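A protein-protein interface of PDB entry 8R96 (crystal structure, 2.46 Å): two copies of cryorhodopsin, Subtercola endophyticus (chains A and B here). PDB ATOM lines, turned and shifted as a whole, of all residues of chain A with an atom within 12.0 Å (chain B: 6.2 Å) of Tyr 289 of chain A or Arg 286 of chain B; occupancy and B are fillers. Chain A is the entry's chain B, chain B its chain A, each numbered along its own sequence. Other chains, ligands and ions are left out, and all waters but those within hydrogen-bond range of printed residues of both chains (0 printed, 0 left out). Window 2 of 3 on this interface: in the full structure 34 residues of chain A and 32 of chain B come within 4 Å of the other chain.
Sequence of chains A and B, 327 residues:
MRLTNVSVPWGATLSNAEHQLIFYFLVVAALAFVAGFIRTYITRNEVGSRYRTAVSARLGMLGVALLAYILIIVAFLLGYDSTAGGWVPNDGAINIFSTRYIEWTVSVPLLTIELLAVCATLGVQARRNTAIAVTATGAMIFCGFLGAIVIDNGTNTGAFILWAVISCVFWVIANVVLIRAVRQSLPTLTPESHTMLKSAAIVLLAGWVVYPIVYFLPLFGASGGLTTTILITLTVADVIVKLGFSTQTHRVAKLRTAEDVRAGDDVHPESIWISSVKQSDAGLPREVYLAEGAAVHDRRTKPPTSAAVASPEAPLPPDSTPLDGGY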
ATOM      1  N   LEU A 284     -20.680 -21.746 -11.686  1.00  0.00           N
ATOM      2  CA  LEU A 284     -19.962 -20.605 -11.059  1.00  0.00           C
ATOM      3  C   LEU A 284     -20.597 -20.313  -9.706  1.00  0.00           C
ATOM      4  O   LEU A 284     -21.782 -20.568  -9.504  1.00  0.00           O
ATOM      5  CB  LEU A 284     -20.044 -19.376 -11.969  1.00  0.00           C
ATOM      6  CG  LEU A 284     -19.380 -19.515 -13.336  1.00  0.00           C
ATOM      7  CD1 LEU A 284     -19.483 -18.216 -14.120  1.00  0.00           C
ATOM      8  CD2 LEU A 284     -17.927 -19.945 -13.194  1.00  0.00           C
ATOM      9  N   PRO A 285     -19.818 -19.788  -8.736  1.00  0.00           N
ATOM     10  CA  PRO A 285     -20.382 -19.253  -7.498  1.00  0.00           C
ATOM     11  C   PRO A 285     -21.248 -18.019  -7.793  1.00  0.00           C
ATOM     12  O   PRO A 285     -20.953 -17.326  -8.755  1.00  0.00           O
ATOM     13  CB  PRO A 285     -19.155 -18.872  -6.654  1.00  0.00           C
ATOM     14  CG  PRO A 285     -17.996 -19.615  -7.299  1.00  0.00           C
ATOM     15  CD  PRO A 285     -18.351 -19.716  -8.767  1.00  0.00           C
ATOM     16  N   ARG A 286     -22.291 -17.788  -6.989  1.00  0.00           N
ATOM     17  CA  ARG A 286     -23.211 -16.629  -7.139  1.00  0.00           C
ATOM     18  C   ARG A 286     -22.402 -15.339  -6.970  1.00  0.00           C
ATOM     19  O   ARG A 286     -21.588 -15.285  -6.033  1.00  0.00           O
ATOM     20  CB  ARG A 286     -24.347 -16.704  -6.114  1.00  0.00           C
ATOM     21  N   GLU A 287     -22.594 -14.359  -7.860  1.00  0.00           N
ATOM     22  CA  GLU A 287     -21.997 -13.003  -7.729  1.00  0.00           C
ATOM     23  C   GLU A 287     -22.594 -12.348  -6.482  1.00  0.00           C
ATOM     24  O   GLU A 287     -23.810 -12.499  -6.270  1.00  0.00           O
ATOM     25  CB  GLU A 287     -22.255 -12.159  -8.977  1.00  0.00           C
ATOM     26  CG  GLU A 287     -21.439 -12.596 -10.175  1.00  0.00           C
ATOM     27  CD  GLU A 287     -21.815 -11.910 -11.477  1.00  0.00           C
ATOM     28  OE1 GLU A 287     -22.650 -10.982 -11.440  1.00  0.00           O
ATOM     29  OE2 GLU A 287     -21.272 -12.309 -12.524  1.00  0.00           O
ATOM     30  N   VAL A 288     -21.764 -11.662  -5.692  1.00  0.00           N
ATOM     31  CA  VAL A 288     -22.113 -11.171  -4.327  1.00  0.00           C
ATOM     32  C   VAL A 288     -21.675  -9.708  -4.201  1.00  0.00           C
ATOM     33  O   VAL A 288     -20.676  -9.329  -4.845  1.00  0.00           O
ATOM     34  CB  VAL A 288     -21.459 -12.055  -3.244  1.00  0.00           C
ATOM     35  CG1 VAL A 288     -21.513 -11.419  -1.864  1.00  0.00           C
ATOM     36  CG2 VAL A 288     -22.077 -13.444  -3.210  1.00  0.00           C
ATOM     37  N   TYR A 289     -22.395  -8.930  -3.384  1.00  0.00           N
ATOM     38  CA  TYR A 289     -22.014  -7.566  -2.935  1.00  0.00           C
ATOM     39  C   TYR A 289     -21.202  -7.656  -1.635  1.00  0.00           C
ATOM     40  O   TYR A 289     -21.085  -8.755  -1.059  1.00  0.00           O
ATOM     41  CB  TYR A 289     -23.257  -6.701  -2.714  1.00  0.00           C
ATOM     42  CG  TYR A 289     -24.042  -6.377  -3.960  1.00  0.00           C
ATOM     43  CD1 TYR A 289     -23.705  -5.294  -4.755  1.00  0.00           C
ATOM     44  CD2 TYR A 289     -25.136  -7.139  -4.334  1.00  0.00           C
ATOM     45  CE1 TYR A 289     -24.425  -4.984  -5.897  1.00  0.00           C
ATOM     46  CE2 TYR A 289     -25.867  -6.843  -5.472  1.00  0.00           C
ATOM     47  CZ  TYR A 289     -25.510  -5.762  -6.258  1.00  0.00           C
ATOM     48  OH  TYR A 289     -26.223  -5.463  -7.383  1.00  0.00           O
ATOM     49  N   LEU A 290     -20.661  -6.521  -1.191  1.00  0.00           N
ATOM     50  CA  LEU A 290     -19.942  -6.382   0.102  1.00  0.00           C
ATOM     51  C   LEU A 290     -20.791  -5.537   1.057  1.00  0.00           C
ATOM     52  O   LEU A 290     -21.373  -4.534   0.599  1.00  0.00           O
ATOM     53  CB  LEU A 290     -18.578  -5.730  -0.147  1.00  0.00           C
ATOM     54  CG  LEU A 290     -17.643  -6.492  -1.085  1.00  0.00           C
ATOM     55  CD1 LEU A 290     -16.321  -5.756  -1.242  1.00  0.00           C
ATOM     56  CD2 LEU A 290     -17.409  -7.909  -0.586  1.00  0.00           C
ATOM     57  N   ALA A 291     -20.864  -5.937   2.330  1.00  0.00           N
ATOM     58  CA  ALA A 291     -21.526  -5.185   3.420  1.00  0.00           C
ATOM     59  C   ALA A 291     -20.802  -3.846   3.630  1.00  0.00           C
ATOM     60  O   ALA A 291     -21.425  -2.913   4.187  1.00  0.00           O
ATOM     61  CB  ALA A 291     -21.537  -6.019   4.677  1.00  0.00           C
ATOM     62  N   GLU A 292     -19.540  -3.757   3.189  1.00  0.00           N
ATOM     63  CA  GLU A 292     -18.664  -2.563   3.353  1.00  0.00           C
ATOM     64  C   GLU A 292     -17.376  -2.744   2.536  1.00  0.00           C
ATOM     65  O   GLU A 292     -16.785  -3.838   2.606  1.00  0.00           O
ATOM     66  CB  GLU A 292     -18.332  -2.355   4.831  1.00  0.00           C
ATOM     67  CG  GLU A 292     -17.699  -1.009   5.125  1.00  0.00           C
ATOM     68  CD  GLU A 292     -18.565   0.174   4.732  1.00  0.00           C
ATOM     69  OE1 GLU A 292     -19.712  -0.054   4.292  1.00  0.00           O
ATOM     70  OE2 GLU A 292     -18.089   1.319   4.867  1.00  0.00           O
ATOM     71  N   GLY A 293     -16.954  -1.704   1.806  1.00  0.00           N
ATOM     72  CA  GLY A 293     -15.736  -1.715   0.971  1.00  0.00           C
ATOM     73  C   GLY A 293     -15.278  -0.311   0.610  1.00  0.00           C
ATOM     74  O   GLY A 293     -15.873   0.654   1.127  1.00  0.00           O
ATOM     75  N   ALA A 294     -14.252  -0.204  -0.243  1.00  0.00           N
ATOM     76  CA  ALA A 294     -13.660   1.066  -0.729  1.00  0.00           C
ATOM     77  C   ALA A 294     -14.754   2.131  -0.849  1.00  0.00           C
ATOM     78  O   ALA A 294     -14.710   3.148  -0.161  1.00  0.00           O
ATOM     79  CB  ALA A 294     -12.970   0.843  -2.052  1.00  0.00           C
ATOM     80  N   GLY B 264     -18.441 -10.708   5.151  1.00  0.00           N
ATOM     81  CA  GLY B 264     -18.808  -9.989   3.915  1.00  0.00           C
ATOM     82  C   GLY B 264     -17.878  -8.819   3.642  1.00  0.00           C
ATOM     83  O   GLY B 264     -18.311  -7.867   2.963  1.00  0.00           O
ATOM     84  N   LEU B 284     -18.171 -14.956  -6.293  1.00  0.00           N
ATOM     85  CA  LEU B 284     -17.630 -14.023  -7.315  1.00  0.00           C
ATOM     86  C   LEU B 284     -17.996 -12.597  -6.921  1.00  0.00           C
ATOM     87  O   LEU B 284     -18.991 -12.373  -6.237  1.00  0.00           O
ATOM     88  CB  LEU B 284     -18.210 -14.376  -8.688  1.00  0.00           C
ATOM     89  CG  LEU B 284     -17.783 -15.733  -9.245  1.00  0.00           C
ATOM     90  CD1 LEU B 284     -18.386 -15.976 -10.619  1.00  0.00           C
ATOM     91  CD2 LEU B 284     -16.269 -15.838  -9.296  1.00  0.00           C
ATOM     92  N   PRO B 285     -17.189 -11.591  -7.323  1.00  0.00           N
ATOM     93  CA  PRO B 285     -17.581 -10.190  -7.184  1.00  0.00           C
ATOM     94  C   PRO B 285     -18.759  -9.864  -8.115  1.00  0.00           C
ATOM     95  O   PRO B 285     -18.919 -10.542  -9.114  1.00  0.00           O
ATOM     96  CB  PRO B 285     -16.330  -9.397  -7.601  1.00  0.00           C
ATOM     97  CG  PRO B 285     -15.199 -10.412  -7.612  1.00  0.00           C
ATOM     98  CD  PRO B 285     -15.850 -11.747  -7.906  1.00  0.00           C
ATOM     99  N   ARG B 286     -19.551  -8.844  -7.779  1.00  0.00           N
ATOM    100  CA  ARG B 286     -20.622  -8.323  -8.671  1.00  0.00           C
ATOM    101  C   ARG B 286     -19.979  -7.800  -9.960  1.00  0.00           C
ATOM    102  O   ARG B 286     -18.929  -7.132  -9.861  1.00  0.00           O
ATOM    103  CB  ARG B 286     -21.425  -7.218  -7.981  1.00  0.00           C
ATOM    104  CG  ARG B 286     -22.820  -7.030  -8.557  1.00  0.00           C
ATOM    105  CD  ARG B 286     -23.713  -8.219  -8.260  1.00  0.00           C
ATOM    106  NE  ARG B 286     -25.001  -8.131  -8.933  1.00  0.00           N
ATOM    107  CZ  ARG B 286     -26.001  -8.987  -8.757  1.00  0.00           C
ATOM    108  NH1 ARG B 286     -27.137  -8.824  -9.416  1.00  0.00           N
ATOM    109  NH2 ARG B 286     -25.865 -10.002  -7.922  1.00  0.00           N
ATOM    110  N   GLU B 287     -20.574  -8.110 -11.116  1.00  0.00           N
ATOM    111  CA  GLU B 287     -20.164  -7.569 -12.440  1.00  0.00           C
ATOM    112  C   GLU B 287     -20.315  -6.044 -12.415  1.00  0.00           C
ATOM    113  O   GLU B 287     -21.283  -5.556 -11.802  1.00  0.00           O
ATOM    114  CB  GLU B 287     -21.000  -8.185 -13.561  1.00  0.00           C
ATOM    115  CG  GLU B 287     -20.659  -9.634 -13.840  1.00  0.00           C
ATOM    116  CD  GLU B 287     -21.476 -10.262 -14.955  1.00  0.00           C
ATOM    117  OE1 GLU B 287     -22.047  -9.506 -15.763  1.00  0.00           O
ATOM    118  OE2 GLU B 287     -21.541 -11.505 -15.011  1.00  0.00           O
ATOM    119  N   VAL B 288     -19.396  -5.327 -13.065  1.00  0.00           N
ATOM    120  CA  VAL B 288     -19.283  -3.841 -12.978  1.00  0.00           C
ATOM    121  C   VAL B 288     -19.400  -3.235 -14.380  1.00  0.00           C
ATOM    122  O   VAL B 288     -18.761  -3.760 -15.316  1.00  0.00           O
ATOM    123  CB  VAL B 288     -17.967  -3.429 -12.290  1.00  0.00           C
ATOM    124  CG1 VAL B 288     -17.775  -1.920 -12.289  1.00  0.00           C
ATOM    125  CG2 VAL B 288     -17.877  -3.981 -10.876  1.00  0.00           C
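O of Gly 264 of chain B sits at hydrogen-bond distance from N of Ala 291 of chain A (3.3 Å). The backbone carbonyl oxygen of Arg 286 of chain A lies within hydrogen-bond range of the backbone NH of Leu 284 of chain B, at 3.4 Å. O of Leu 284 of chain B sits at hydrogen-bond distance from N of Val 288 of chain A, at 2.9 Å. N of Arg 286 of chain B is in hydrogen-bond range of O of Val 288 of chain A (3.2 Å). The guanidinium group (NE) of Arg 286 of chain B sits at hydrogen-bond distance from the side-chain hydroxyl (OH) of Tyr 289 of chain A, at 3.3 Å. OE2 of Glu 287 of chain B sits close to OE2 of Glu 287 of chain A (2.6 Å).
Leu 284 of chain B touches Pro 285 of chain A. Glu 287 of chain A touches Leu 284 of chain B. O of Pro 285 of chain B touches CG of Glu 287 of chain A (3.4 Å). Arg 286 of chain B touches Glu 287 of chain A. Pro 285 of chain B touches Val 288 of chain A (C to O, 3.8 Å). Leu 290 of chain A touches Gly 264 of chain B.
Of the printed residues of chain B, Tyr 289 of chain A touches Arg 286. Arg 286 of chain B touches just these residues of chain A: Glu 287 (3.6 Å), Val 288 (3.2 Å) and Tyr 289 (3.3 Å). Gly 264 of chain B touches just these residues of chain A: Leu 290 (3.6 Å) and Ala 291 (3.3 Å). Pro 285 of chain B touches just these residues of chain A: Glu 287 and Val 288. Of chain A, only Glu 287 comes within 4 Å of Glu 287 of chain B. No residue of chain A comes within 4 Å of Val 288 of chain B. Of the printed residues of chain B, Glu 287 of chain A touches Leu 284 (3.4 Å), Pro 285 (3.4 Å), Arg 286 (3.6 Å) and Glu 287 (2.6 Å). Of the printed residues of chain B, Leu 290 of chain A touches Gly 264. The nearest residue of chain A that does not touch Arg 286 of chain B is Arg 286 of chain A (6.4 Å). The nearest printed residue of chain B that does not touch Pro 285 of chain A is Pro 285 of chain B (7.0 Å).
Hydrophobic or aromatic side chains of chain A that line the printed part of chain B: Val 288, Tyr 289 and Leu 290. Among the printed residues, 12 pairs touch across the chains. Among the printed residues, no Asp or Glu carboxylate lies within 4 Å of a Lys or Arg side-chain nitrogen of the other chain.
Glu 287 of chain A touches Leu 284 of chain B, but with the chains exchanged Leu 284 of chain A does not touch Glu 287 of chain B (7.1 Å). Glu 287 of chain A touches Pro 285 of chain B, but with the chains exchanged Pro 285 of chain A does not touch Glu 287 of chain B (8.6 Å). Glu 287 of chain A touches Arg 286 of chain B, but with the chains exchanged Arg 286 of chain A does not touch Glu 287 of chain B (8.5 Å). Val 288 of chain A touches Pro 285 of chain B, but with the chains exchanged Pro 285 of chain A does not touch Val 288 of chain B (12.8 Å). 5 positions are printed for both chains. Of the 12 pairs that touch across the chains among the printed residues, 1 has its exchanged pair printed and touching as well.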
